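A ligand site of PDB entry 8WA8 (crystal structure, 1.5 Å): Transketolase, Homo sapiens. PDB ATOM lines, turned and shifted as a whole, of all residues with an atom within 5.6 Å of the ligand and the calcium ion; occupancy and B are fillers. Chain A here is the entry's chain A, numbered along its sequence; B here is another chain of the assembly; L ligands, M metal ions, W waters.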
ATOM      1  N   HIS A  37     -11.687  28.356  -5.920  1.00  0.00           N
ATOM      2  CA  HIS A  37     -12.272  27.231  -5.186  1.00  0.00           C
ATOM      3  C   HIS A  37     -13.783  27.386  -5.049  1.00  0.00           C
ATOM      4  O   HIS A  37     -14.320  27.460  -3.938  1.00  0.00           O
ATOM      5  CB  HIS A  37     -11.635  27.127  -3.799  1.00  0.00           C
ATOM      6  CG  HIS A  37     -10.152  26.905  -3.819  1.00  0.00           C
ATOM      7  ND1 HIS A  37      -9.252  27.866  -4.232  1.00  0.00           N
ATOM      8  CD2 HIS A  37      -9.413  25.829  -3.471  1.00  0.00           C
ATOM      9  CE1 HIS A  37      -8.021  27.387  -4.141  1.00  0.00           C
ATOM     10  NE2 HIS A  37      -8.091  26.151  -3.666  1.00  0.00           N
ATOM     11  N   SER A  40     -15.666  25.104  -2.564  1.00  0.00           N
ATOM     12  CA  SER A  40     -15.448  25.442  -1.159  1.00  0.00           C
ATOM     13  C   SER A  40     -16.258  26.657  -0.737  1.00  0.00           C
ATOM     14  O   SER A  40     -16.624  26.780   0.442  1.00  0.00           O
ATOM     15  CB  SER A  40     -13.961  25.734  -0.912  1.00  0.00           C
ATOM     16  OG  SER A  40     -13.141  24.634  -1.266  1.00  0.00           O
ATOM     17  N   SER A  43     -20.261  25.329  -0.294  1.00  0.00           N
ATOM     18  CA  SER A  43     -20.700  24.660   0.923  1.00  0.00           C
ATOM     19  C   SER A  43     -21.000  25.636   2.041  1.00  0.00           C
ATOM     20  O   SER A  43     -21.762  25.308   2.963  1.00  0.00           O
ATOM     21  CB  SER A  43     -19.682  23.601   1.371  1.00  0.00           C
ATOM     22  OG  SER A  43     -18.438  24.172   1.658  1.00  0.00           O
ATOM     23  N   LYS A  75     -10.892  29.192   6.624  1.00  0.00           N
ATOM     24  CA  LYS A  75     -10.713  28.477   5.351  1.00  0.00           C
ATOM     25  C   LYS A  75     -10.588  29.521   4.239  1.00  0.00           C
ATOM     26  O   LYS A  75     -11.522  29.778   3.463  1.00  0.00           O
ATOM     27  CB  LYS A  75     -11.813  27.453   5.106  1.00  0.00           C
ATOM     28  CG  LYS A  75     -13.232  27.915   5.436  1.00  0.00           C
ATOM     29  CD  LYS A  75     -14.287  26.865   4.983  1.00  0.00           C
ATOM     30  CE  LYS A  75     -14.663  27.086   3.523  1.00  0.00           C
ATOM     31  NZ  LYS A  75     -15.541  25.996   2.982  1.00  0.00           N
ATOM     32  N   HIS A  77      -9.210  29.938   1.385  1.00  0.00           N
ATOM     33  CA  HIS A  77      -9.420  29.701  -0.043  1.00  0.00           C
ATOM     34  C   HIS A  77     -10.869  29.923  -0.470  1.00  0.00           C
ATOM     35  O   HIS A  77     -11.136  29.953  -1.676  1.00  0.00           O
ATOM     36  CB  HIS A  77      -8.948  28.297  -0.424  1.00  0.00           C
ATOM     37  CG  HIS A  77      -9.549  27.217   0.425  1.00  0.00           C
ATOM     38  ND1 HIS A  77      -9.199  27.026   1.743  1.00  0.00           N
ATOM     39  CD2 HIS A  77     -10.487  26.288   0.135  1.00  0.00           C
ATOM     40  CE1 HIS A  77      -9.897  26.017   2.230  1.00  0.00           C
ATOM     41  NE2 HIS A  77     -10.687  25.547   1.276  1.00  0.00           N
ATOM     42  N   GLY A 123      -5.056  31.368   4.711  1.00  0.00           N
ATOM     43  CA  GLY A 123      -4.527  30.690   3.553  1.00  0.00           C
ATOM     44  C   GLY A 123      -3.681  29.524   4.014  1.00  0.00           C
ATOM     45  O   GLY A 123      -3.659  28.474   3.371  1.00  0.00           O
ATOM     46  N   SER A 124      -2.987  29.706   5.131  1.00  0.00           N
ATOM     47  CA  SER A 124      -2.377  28.575   5.829  1.00  0.00           C
ATOM     48  C   SER A 124      -3.405  28.080   6.835  1.00  0.00           C
ATOM     49  O   SER A 124      -3.717  28.782   7.807  1.00  0.00           O
ATOM     50  CB  SER A 124      -1.083  29.000   6.524  1.00  0.00           C
ATOM     51  OG  SER A 124      -0.585  27.897   7.254  1.00  0.00           O
ATOM     52  N   LEU A 125      -3.945  26.888   6.579  1.00  0.00           N
ATOM     53  CA  LEU A 125      -5.102  26.405   7.318  1.00  0.00           C
ATOM     54  C   LEU A 125      -4.772  26.199   8.802  1.00  0.00           C
ATOM     55  O   LEU A 125      -3.634  25.878   9.173  1.00  0.00           O
ATOM     56  CB  LEU A 125      -5.576  25.082   6.734  1.00  0.00           C
ATOM     57  CG  LEU A 125      -6.190  25.207   5.341  1.00  0.00           C
ATOM     58  CD1 LEU A 125      -6.391  23.822   4.735  1.00  0.00           C
ATOM     59  CD2 LEU A 125      -7.509  25.930   5.434  1.00  0.00           C
ATOM     60  N   GLY A 154     -12.938  24.910   7.795  1.00  0.00           N
ATOM     61  CA  GLY A 154     -13.245  23.705   7.052  1.00  0.00           C
ATOM     62  C   GLY A 154     -13.043  22.442   7.886  1.00  0.00           C
ATOM     63  O   GLY A 154     -12.476  22.477   8.989  1.00  0.00           O
ATOM     64  N   ASP A 155     -13.485  21.311   7.347  1.00  0.00           N
ATOM     65  CA  ASP A 155     -13.330  20.081   8.124  1.00  0.00           C
ATOM     66  C   ASP A 155     -11.945  19.451   7.964  1.00  0.00           C
ATOM     67  O   ASP A 155     -11.371  18.949   8.947  1.00  0.00           O
ATOM     68  CB  ASP A 155     -14.499  19.082   7.918  1.00  0.00           C
ATOM     69  CG  ASP A 155     -14.728  18.669   6.461  1.00  0.00           C
ATOM     70  OD1 ASP A 155     -14.153  19.242   5.532  1.00  0.00           O
ATOM     71  OD2 ASP A 155     -15.551  17.750   6.261  1.00  0.00           O
ATOM     72  N   GLY A 156     -11.388  19.470   6.749  1.00  0.00           N
ATOM     73  CA  GLY A 156     -10.001  19.049   6.596  1.00  0.00           C
ATOM     74  C   GLY A 156      -9.073  19.875   7.467  1.00  0.00           C
ATOM     75  O   GLY A 156      -8.144  19.349   8.093  1.00  0.00           O
ATOM     76  N   GLU A 157      -9.365  21.175   7.577  1.00  0.00           N
ATOM     77  CA  GLU A 157      -8.592  22.088   8.409  1.00  0.00           C
ATOM     78  C   GLU A 157      -8.520  21.650   9.871  1.00  0.00           C
ATOM     79  O   GLU A 157      -7.540  21.948  10.572  1.00  0.00           O
ATOM     80  CB  GLU A 157      -9.253  23.470   8.298  1.00  0.00           C
ATOM     81  CG  GLU A 157      -8.656  24.529   9.160  1.00  0.00           C
ATOM     82  CD  GLU A 157      -9.165  25.919   8.814  1.00  0.00           C
ATOM     83  OE1 GLU A 157     -10.289  26.061   8.254  1.00  0.00           O
ATOM     84  OE2 GLU A 157      -8.421  26.865   9.110  1.00  0.00           O
ATOM     85  N   LEU A 158      -9.547  20.946  10.358  1.00  0.00           N
ATOM     86  CA  LEU A 158      -9.594  20.503  11.754  1.00  0.00           C
ATOM     87  C   LEU A 158      -8.548  19.447  12.066  1.00  0.00           C
ATOM     88  O   LEU A 158      -8.399  19.082  13.243  1.00  0.00           O
ATOM     89  CB  LEU A 158     -10.989  20.001  12.128  1.00  0.00           C
ATOM     90  CG  LEU A 158     -12.088  21.020  11.820  1.00  0.00           C
ATOM     91  CD1 LEU A 158     -13.470  20.448  12.094  1.00  0.00           C
ATOM     92  CD2 LEU A 158     -11.875  22.319  12.601  1.00  0.00           C
ATOM     93  N   GLU A 160      -5.442  20.141  11.804  1.00  0.00           N
ATOM     94  CA  GLU A 160      -4.293  20.895  12.296  1.00  0.00           C
ATOM     95  C   GLU A 160      -4.333  21.013  13.816  1.00  0.00           C
ATOM     96  O   GLU A 160      -5.327  21.453  14.395  1.00  0.00           O
ATOM     97  CB  GLU A 160      -4.254  22.303  11.701  1.00  0.00           C
ATOM     98  CG  GLU A 160      -3.883  22.376  10.227  1.00  0.00           C
ATOM     99  CD  GLU A 160      -2.418  22.104   9.945  1.00  0.00           C
ATOM    100  OE1 GLU A 160      -1.632  21.797  10.867  1.00  0.00           O
ATOM    101  OE2 GLU A 160      -2.034  22.223   8.767  1.00  0.00           O
ATOM    102  N   ASP A 183     -17.507  23.908   8.749  1.00  0.00           N
ATOM    103  CA  ASP A 183     -18.109  23.580   7.459  1.00  0.00           C
ATOM    104  C   ASP A 183     -17.774  22.117   7.161  1.00  0.00           C
ATOM    105  O   ASP A 183     -16.766  21.806   6.529  1.00  0.00           O
ATOM    106  CB  ASP A 183     -17.588  24.544   6.402  1.00  0.00           C
ATOM    107  CG  ASP A 183     -18.212  24.327   5.015  1.00  0.00           C
ATOM    108  OD1 ASP A 183     -19.005  23.375   4.841  1.00  0.00           O
ATOM    109  OD2 ASP A 183     -17.908  25.132   4.099  1.00  0.00           O
ATOM    110  N   ASN A 185     -18.167  19.583   5.142  1.00  0.00           N
ATOM    111  CA  ASN A 185     -18.611  19.236   3.799  1.00  0.00           C
ATOM    112  C   ASN A 185     -18.044  17.910   3.296  1.00  0.00           C
ATOM    113  O   ASN A 185     -18.127  17.630   2.096  1.00  0.00           O
ATOM    114  CB  ASN A 185     -18.356  20.378   2.802  1.00  0.00           C
ATOM    115  CG  ASN A 185     -16.884  20.668   2.598  1.00  0.00           C
ATOM    116  OD1 ASN A 185     -16.013  19.870   2.965  1.00  0.00           O
ATOM    117  ND2 ASN A 185     -16.602  21.836   2.026  1.00  0.00           N
ATOM    118  N   ARG A 186     -17.464  17.118   4.199  1.00  0.00           N
ATOM    119  CA  ARG A 186     -17.096  15.710   3.977  1.00  0.00           C
ATOM    120  C   ARG A 186     -15.745  15.534   3.305  1.00  0.00           C
ATOM    121  O   ARG A 186     -15.081  14.503   3.505  1.00  0.00           O
ATOM    122  CB  ARG A 186     -18.191  14.936   3.226  1.00  0.00           C
ATOM    123  CG  ARG A 186     -18.048  13.431   3.363  1.00  0.00           C
ATOM    124  CD  ARG A 186     -19.150  12.677   2.619  1.00  0.00           C
ATOM    125  NE  ARG A 186     -19.065  12.862   1.171  1.00  0.00           N
ATOM    126  CZ  ARG A 186     -18.258  12.160   0.384  1.00  0.00           C
ATOM    127  NH1 ARG A 186     -17.410  11.258   0.865  1.00  0.00           N
ATOM    128  NH2 ARG A 186     -18.306  12.366  -0.936  1.00  0.00           N
ATOM    129  N   LEU A 187     -15.314  16.508   2.499  1.00  0.00           N
ATOM    130  CA  LEU A 187     -14.173  16.338   1.617  1.00  0.00           C
ATOM    131  C   LEU A 187     -13.071  17.330   1.929  1.00  0.00           C
ATOM    132  O   LEU A 187     -13.327  18.480   2.315  1.00  0.00           O
ATOM    133  CB  LEU A 187     -14.607  16.513   0.142  1.00  0.00           C
ATOM    134  CG  LEU A 187     -15.645  15.505  -0.356  1.00  0.00           C
ATOM    135  CD1 LEU A 187     -16.050  15.798  -1.795  1.00  0.00           C
ATOM    136  CD2 LEU A 187     -15.111  14.079  -0.223  1.00  0.00           C
ATOM    137  N   GLY A 188     -11.834  16.877   1.765  1.00  0.00           N
ATOM    138  CA  GLY A 188     -10.665  17.738   1.749  1.00  0.00           C
ATOM    139  C   GLY A 188     -10.241  18.062   0.331  1.00  0.00           C
ATOM    140  O   GLY A 188     -11.066  18.140  -0.595  1.00  0.00           O
ATOM    141  N   GLN A 189      -8.928  18.259   0.155  1.00  0.00           N
ATOM    142  CA  GLN A 189      -8.404  18.584  -1.164  1.00  0.00           C
ATOM    143  C   GLN A 189      -8.293  17.357  -2.066  1.00  0.00           C
ATOM    144  O   GLN A 189      -8.648  17.421  -3.258  1.00  0.00           O
ATOM    145  CB  GLN A 189      -7.030  19.245  -1.041  1.00  0.00           C
ATOM    146  CG  GLN A 189      -6.319  19.334  -2.393  1.00  0.00           C
ATOM    147  CD  GLN A 189      -5.112  20.230  -2.369  1.00  0.00           C
ATOM    148  OE1 GLN A 189      -5.071  21.222  -1.640  1.00  0.00           O
ATOM    149  NE2 GLN A 189      -4.106  19.899  -3.174  1.00  0.00           N
ATOM    150  N   ALA A 193     -12.306  14.020   4.077  1.00  0.00           N
ATOM    151  CA  ALA A 193     -11.739  14.297   5.390  1.00  0.00           C
ATOM    152  C   ALA A 193     -11.888  13.063   6.276  1.00  0.00           C
ATOM    153  O   ALA A 193     -12.828  12.281   6.092  1.00  0.00           O
ATOM    154  CB  ALA A 193     -12.442  15.498   6.034  1.00  0.00           C
ATOM    155  N   LYS A 244     -19.953  19.750  -0.227  1.00  0.00           N
ATOM    156  CA  LYS A 244     -19.030  20.536  -1.028  1.00  0.00           C
ATOM    157  C   LYS A 244     -19.634  20.714  -2.419  1.00  0.00           C
ATOM    158  O   LYS A 244     -20.185  19.774  -2.988  1.00  0.00           O
ATOM    159  CB  LYS A 244     -17.688  19.817  -1.123  1.00  0.00           C
ATOM    160  CG  LYS A 244     -16.521  20.726  -1.434  1.00  0.00           C
ATOM    161  CD  LYS A 244     -15.186  20.100  -1.001  1.00  0.00           C
ATOM    162  CE  LYS A 244     -14.011  21.020  -1.310  1.00  0.00           C
ATOM    163  NZ  LYS A 244     -12.749  20.602  -0.576  1.00  0.00           N
ATOM    164  N   HIS A 258     -11.829  19.992  -5.849  1.00  0.00           N
ATOM    165  CA  HIS A 258     -11.273  21.004  -4.970  1.00  0.00           C
ATOM    166  C   HIS A 258     -10.326  21.906  -5.748  1.00  0.00           C
ATOM    167  O   HIS A 258      -9.426  21.427  -6.428  1.00  0.00           O
ATOM    168  CB  HIS A 258     -10.496  20.357  -3.818  1.00  0.00           C
ATOM    169  CG  HIS A 258      -9.899  21.366  -2.885  1.00  0.00           C
ATOM    170  ND1 HIS A 258     -10.599  21.900  -1.824  1.00  0.00           N
ATOM    171  CD2 HIS A 258      -8.698  21.979  -2.907  1.00  0.00           C
ATOM    172  CE1 HIS A 258      -9.823  22.773  -1.202  1.00  0.00           C
ATOM    173  NE2 HIS A 258      -8.666  22.845  -1.842  1.00  0.00           N
ATOM    174  N   ASP A 398       5.182  29.121  10.977  1.00  0.00           N
ATOM    175  CA  ASP A 398       4.132  29.395   9.991  1.00  0.00           C
ATOM    176  C   ASP A 398       3.189  30.489  10.489  1.00  0.00           C
ATOM    177  O   ASP A 398       2.728  31.341   9.712  1.00  0.00           O
ATOM    178  CB  ASP A 398       3.372  28.097   9.681  1.00  0.00           C
ATOM    179  CG  ASP A 398       2.467  28.198   8.451  1.00  0.00           C
ATOM    180  OD1 ASP A 398       2.659  29.078   7.589  1.00  0.00           O
ATOM    181  OD2 ASP A 398       1.548  27.354   8.338  1.00  0.00           O
ATOM    182  N   GLY B 340       0.489  15.458   2.939  1.00  0.00           N
ATOM    183  CA  GLY B 340      -0.507  16.097   3.775  1.00  0.00           C
ATOM    184  C   GLY B 340      -1.720  16.622   3.033  1.00  0.00           C
ATOM    185  O   GLY B 340      -1.925  17.843   2.982  1.00  0.00           O
ATOM    186  N   ASP B 341      -2.544  15.729   2.489  1.00  0.00           N
ATOM    187  CA  ASP B 341      -3.721  16.097   1.698  1.00  0.00           C
ATOM    188  C   ASP B 341      -3.377  16.988   0.510  1.00  0.00           C
ATOM    189  O   ASP B 341      -4.206  17.787   0.056  1.00  0.00           O
ATOM    190  CB  ASP B 341      -4.835  16.714   2.549  1.00  0.00           C
ATOM    191  CG  ASP B 341      -6.186  16.796   1.821  1.00  0.00           C
ATOM    192  OD1 ASP B 341      -6.436  15.962   0.923  1.00  0.00           O
ATOM    193  OD2 ASP B 341      -6.980  17.703   2.138  1.00  0.00           O
ATOM    194  N   THR B 342      -2.151  16.869  -0.029  1.00  0.00           N
ATOM    195  CA  THR B 342      -1.766  17.661  -1.193  1.00  0.00           C
ATOM    196  C   THR B 342      -1.247  16.802  -2.345  1.00  0.00           C
ATOM    197  O   THR B 342      -0.593  17.328  -3.243  1.00  0.00           O
ATOM    198  CB  THR B 342      -0.751  18.765  -0.835  1.00  0.00           C
ATOM    199  OG1 THR B 342       0.345  18.195  -0.099  1.00  0.00           O
ATOM    200  CG2 THR B 342      -1.404  19.858   0.010  1.00  0.00           C
ATOM    201  N   ILE B 364      -4.146  17.119   6.818  1.00  0.00           N
ATOM    202  CA  ILE B 364      -3.627  18.479   6.942  1.00  0.00           C
ATOM    203  C   ILE B 364      -2.997  18.636   8.323  1.00  0.00           C
ATOM    204  O   ILE B 364      -3.594  19.212   9.241  1.00  0.00           O
ATOM    205  CB  ILE B 364      -4.727  19.514   6.648  1.00  0.00           C
ATOM    206  CG1 ILE B 364      -5.370  19.182   5.298  1.00  0.00           C
ATOM    207  CG2 ILE B 364      -4.133  20.920   6.579  1.00  0.00           C
ATOM    208  CD1 ILE B 364      -6.559  20.084   4.933  1.00  0.00           C
ATOM    209  N   GLU B 366       1.042  18.935   9.156  1.00  0.00           N
ATOM    210  CA  GLU B 366       2.428  18.858   8.707  1.00  0.00           C
ATOM    211  C   GLU B 366       3.370  18.499   9.854  1.00  0.00           C
ATOM    212  O   GLU B 366       4.365  17.800   9.640  1.00  0.00           O
ATOM    213  CB  GLU B 366       2.848  20.181   8.081  1.00  0.00           C
ATOM    214  CG  GLU B 366       2.097  20.558   6.813  1.00  0.00           C
ATOM    215  CD  GLU B 366       0.702  21.100   7.056  1.00  0.00           C
ATOM    216  OE1 GLU B 366       0.375  21.468   8.205  1.00  0.00           O
ATOM    217  OE2 GLU B 366      -0.059  21.181   6.088  1.00  0.00           O
ATOM    218  N   THR B 388       4.623  18.245   0.738  1.00  0.00           N
ATOM    219  CA  THR B 388       3.544  19.224   0.794  1.00  0.00           C
ATOM    220  C   THR B 388       4.052  20.444   0.035  1.00  0.00           C
ATOM    221  O   THR B 388       5.121  20.405  -0.579  1.00  0.00           O
ATOM    222  CB  THR B 388       3.111  19.527   2.231  1.00  0.00           C
ATOM    223  OG1 THR B 388       2.032  20.469   2.224  1.00  0.00           O
ATOM    224  CG2 THR B 388       4.265  20.122   3.053  1.00  0.00           C
ATOM    225  N   PHE B 389       3.300  21.533   0.092  1.00  0.00           N
ATOM    226  CA  PHE B 389       3.838  22.794  -0.392  1.00  0.00           C
ATOM    227  C   PHE B 389       4.991  23.218   0.516  1.00  0.00           C
ATOM    228  O   PHE B 389       4.894  23.129   1.750  1.00  0.00           O
ATOM    229  CB  PHE B 389       2.779  23.896  -0.336  1.00  0.00           C
ATOM    230  CG  PHE B 389       1.658  23.748  -1.324  1.00  0.00           C
ATOM    231  CD1 PHE B 389       1.397  22.547  -1.948  1.00  0.00           C
ATOM    232  CD2 PHE B 389       0.870  24.844  -1.625  1.00  0.00           C
ATOM    233  CE1 PHE B 389       0.366  22.428  -2.854  1.00  0.00           C
ATOM    234  CE2 PHE B 389      -0.168  24.730  -2.537  1.00  0.00           C
ATOM    235  CZ  PHE B 389      -0.417  23.519  -3.148  1.00  0.00           C
ATOM    236  N   PHE B 392       4.342  25.221   3.670  1.00  0.00           N
ATOM    237  CA  PHE B 392       3.754  24.585   4.848  1.00  0.00           C
ATOM    238  C   PHE B 392       4.737  23.738   5.628  1.00  0.00           C
ATOM    239  O   PHE B 392       4.414  23.301   6.732  1.00  0.00           O
ATOM    240  CB  PHE B 392       2.476  23.832   4.447  1.00  0.00           C
ATOM    241  CG  PHE B 392       1.489  24.715   3.748  1.00  0.00           C
ATOM    242  CD1 PHE B 392       1.240  26.002   4.222  1.00  0.00           C
ATOM    243  CD2 PHE B 392       0.853  24.284   2.599  1.00  0.00           C
ATOM    244  CE1 PHE B 392       0.365  26.838   3.570  1.00  0.00           C
ATOM    245  CE2 PHE B 392      -0.033  25.131   1.935  1.00  0.00           C
ATOM    246  CZ  PHE B 392      -0.270  26.408   2.422  1.00  0.00           C
ATOM    247  N   ARG B 395       5.382  25.155   9.030  1.00  0.00           N
ATOM    248  CA  ARG B 395       4.543  24.669  10.120  1.00  0.00           C
ATOM    249  C   ARG B 395       5.242  23.589  10.951  1.00  0.00           C
ATOM    250  O   ARG B 395       4.890  23.384  12.123  1.00  0.00           O
ATOM    251  CB  ARG B 395       3.225  24.140   9.539  1.00  0.00           C
ATOM    252  CG  ARG B 395       2.141  23.862  10.566  1.00  0.00           C
ATOM    253  CD  ARG B 395       1.658  25.164  11.210  1.00  0.00           C
ATOM    254  NE  ARG B 395       0.274  25.058  11.638  1.00  0.00           N
ATOM    255  CZ  ARG B 395      -0.769  25.424  10.911  1.00  0.00           C
ATOM    256  NH1 ARG B 395      -0.632  25.965   9.701  1.00  0.00           N
ATOM    257  NH2 ARG B 395      -1.986  25.252  11.399  1.00  0.00           N
ATOM    258  N   GLN B 428       0.540  30.775   0.064  1.00  0.00           N
ATOM    259  CA  GLN B 428       0.965  29.513  -0.525  1.00  0.00           C
ATOM    260  C   GLN B 428       2.371  29.572  -1.108  1.00  0.00           C
ATOM    261  O   GLN B 428       2.857  28.547  -1.596  1.00  0.00           O
ATOM    262  CB  GLN B 428      -0.028  29.092  -1.631  1.00  0.00           C
ATOM    263  CG  GLN B 428      -1.499  29.367  -1.308  1.00  0.00           C
ATOM    264  CD  GLN B 428      -2.031  28.507  -0.187  1.00  0.00           C
ATOM    265  OE1 GLN B 428      -2.542  29.023   0.808  1.00  0.00           O
ATOM    266  NE2 GLN B 428      -1.927  27.190  -0.341  1.00  0.00           N
HETATM  267  N1  LIG L   1      -1.600  22.864   4.691  1.00  0.00           N
HETATM  268  C1  LIG L   1      -1.882  24.085   5.175  1.00  0.00           C
HETATM  269  C2  LIG L   1      -1.392  24.433   6.538  1.00  0.00           C
HETATM  270  N2  LIG L   1      -2.588  25.027   4.528  1.00  0.00           N
HETATM  271  C3  LIG L   1      -3.032  24.741   3.298  1.00  0.00           C
HETATM  272  N3  LIG L   1      -3.709  25.706   2.659  1.00  0.00           N
HETATM  273  C4  LIG L   1      -2.783  23.466   2.690  1.00  0.00           C
HETATM  274  C5  LIG L   1      -2.067  22.581   3.469  1.00  0.00           C
HETATM  275  C6  LIG L   1      -3.264  23.101   1.303  1.00  0.00           C
HETATM  276  N4  LIG L   1      -4.739  23.171   1.178  1.00  0.00           N
HETATM  277  C7  LIG L   1      -5.404  24.263   0.820  1.00  0.00           C
HETATM  278  S1  LIG L   1      -7.069  24.035   0.858  1.00  0.00           S
HETATM  279  C8  LIG L   1      -6.846  22.401   1.358  1.00  0.00           C
HETATM  280  C9  LIG L   1      -5.553  22.104   1.522  1.00  0.00           C
HETATM  281  C10 LIG L   1      -4.952  20.801   1.945  1.00  0.00           C
HETATM  282  C11 LIG L   1      -8.038  21.551   1.660  1.00  0.00           C
HETATM  283  C12 LIG L   1      -8.986  22.270   2.579  1.00  0.00           C
HETATM  284  O1  LIG L   1      -9.993  21.354   3.050  1.00  0.00           O
HETATM  285  P1  LIG L   1     -11.114  21.770   4.065  1.00  0.00           P
HETATM  286  O2  LIG L   1     -11.935  20.560   4.267  1.00  0.00           O
HETATM  287  O3  LIG L   1     -10.492  22.431   5.285  1.00  0.00           O
HETATM  288  O4  LIG L   1     -11.901  22.874   3.258  1.00  0.00           O
HETATM  289  P2  LIG L   1     -13.051  22.954   2.162  1.00  0.00           P
HETATM  290  O5  LIG L   1     -12.462  23.552   0.920  1.00  0.00           O
HETATM  291  O6  LIG L   1     -14.134  23.777   2.830  1.00  0.00           O
HETATM  292  O7  LIG L   1     -13.491  21.525   1.972  1.00  0.00           O
HETATM  293 CA    CA M   1     -13.920  20.105   3.580  1.00  0.00          CA
HETATM  294  O   HOH W   1      -0.014  19.772   3.682  1.00  0.00           O
HETATM  295  O   HOH W   2     -14.763  21.939   4.674  1.00  0.00           O
HETATM  296  O   HOH W   3      -5.433  27.366   0.681  1.00  0.00           O
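Three residues have an atom within 4 Å of the calcium ion: Asp 155, Asn 185 and Leu 187. The nearest printed residue that does not touch the calcium ion is Gly 156 (4.1 Å).
Water W2 lies within hydrogen-bond range of an oxygen (O6) of the ligand (2.7 Å), the backbone carbonyl oxygen of Asp 183 (2.7 Å), the backbone NH of Asp 155 (3.0 Å) and the side-chain amide nitrogen of Asn 185 (3.2 Å). Water W3 lies within hydrogen-bond range of N3 of the ligand (3.1 Å), OE1 of Gln 428 of chain B (3.3 Å) and O of Gly 123 (3.4 Å). Water W1 lies within hydrogen-bond range of the side-chain hydroxyl (OG1) of Thr 388 of chain B (2.6 Å), the side-chain carboxylate (OE2) of Glu 366 of chain B (2.8 Å) and the backbone carbonyl oxygen (O) of Gly 340 of chain B (2.8 Å).
The side-chain carboxylate of Glu 366 of chain B is in hydrogen-bond range of a nitrogen (N1) of the ligand (2.7 Å). O6 of the ligand lies within salt-bridge range of NZ of Lys 75. The side-chain hydroxyl (OG) of Ser 40 is in hydrogen-bond range of an oxygen (O5) of the ligand, at 2.5 Å. O of Gly 123 lies within hydrogen-bond range of N3 of the ligand (2.9 Å). An oxygen (O3) of the ligand lies within hydrogen-bond range of the backbone NH of Glu 157, at 2.8 Å. N of Leu 125 is in hydrogen-bond range of N2 of the ligand, at 3.1 Å. O5 of the ligand is in hydrogen-bond range of NE2 of His 77, at 2.7 Å. A sulfur (S1) of the ligand sits close to a ring nitrogen (NE2) of His 258, at 3.4 Å. The backbone NH of Gly 156 lies within hydrogen-bond range of an oxygen (O3) of the ligand, 3.4 Å away. O5 of the ligand lies within salt-bridge range of NZ of Lys 244, 3.3 Å away.
OG of Ser 43 sits at hydrogen-bond distance from ND2 of Asn 185, at 3.0 Å. The backbone NH of Asp 155 lies within hydrogen-bond range of the backbone carbonyl oxygen of Asp 183 (3.4 Å). The side-chain amino group of Lys 75 sits at hydrogen-bond distance from the backbone carbonyl oxygen of Ser 40 (2.9 Å). ND1 of His 258 sits at hydrogen-bond distance from NZ of Lys 244 (2.8 Å). The side-chain hydroxyl (OG) of Ser 124 lies within hydrogen-bond range of the side-chain carboxylate (OD2) of Asp 398. NH1 of Arg 395 of chain B lies within salt-bridge range of OD2 of Asp 398 (2.9 Å). NZ of Lys 75 lies within salt-bridge range of OD2 of Asp 183 (2.8 Å). The side-chain carboxylate (OD2) of Asp 341 of chain B is in hydrogen-bond range of the backbone NH (N) of Gln 189 (2.8 Å).
The side-chain amide oxygen (OE1) of Gln 189 lies close to a nitrogen (N4) of the ligand (3.4 Å). Ser 124 touches the ligand. Gly 154 touches the ligand (CA to O3, 3.5 Å). OE2 of Glu 160 touches C2 of the ligand, at 3.2 Å. Gly 188 touches the ligand. O of Asp 341 of chain B touches C10 of the ligand, 3.6 Å away. Thr 342 of chain B touches the ligand. Ile 364 of chain B touches the ligand (CD1 to C10, 3.5 Å). Phe 392 of chain B touches the ligand. NH1 of Arg 395 of chain B touches C2 of the ligand, at 3.6 Å. Gln 428 of chain B touches the ligand (NE2 to N3, 3.8 Å). Hydrophobic or aromatic side chains within 4 Å of the ligand: His 77, Leu 125, His 258, Ile 364 of chain B and Phe 392 of chain B. Within 4 Å of the ligand: Ser 40, Lys 75, His 77, Gly 123, Ser 124, Leu 125, Gly 154, Asp 155, Gly 156, Glu 157, Glu 160, Asn 185, Leu 187, Gly 188, Gln 189, Lys 244, His 258, Asp 341 of chain B, Thr 342 of chain B, Ile 364 of chain B, Glu 366 of chain B, Phe 392 of chain B, Arg 395 of chain B and Gln 428 of chain B. The nearest printed residue that does not touch the ligand is Asp 183 (4.2 Å).
The calcium ion is bound by O of Leu 187 (2.1 Å), OD1 of Asp 155 (2.1 Å), O2 of the ligand (2.1 Å), O7 of the ligand (2.2 Å), OD1 of Asn 185 (2.2 Å) and water W2 (2.3 Å).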
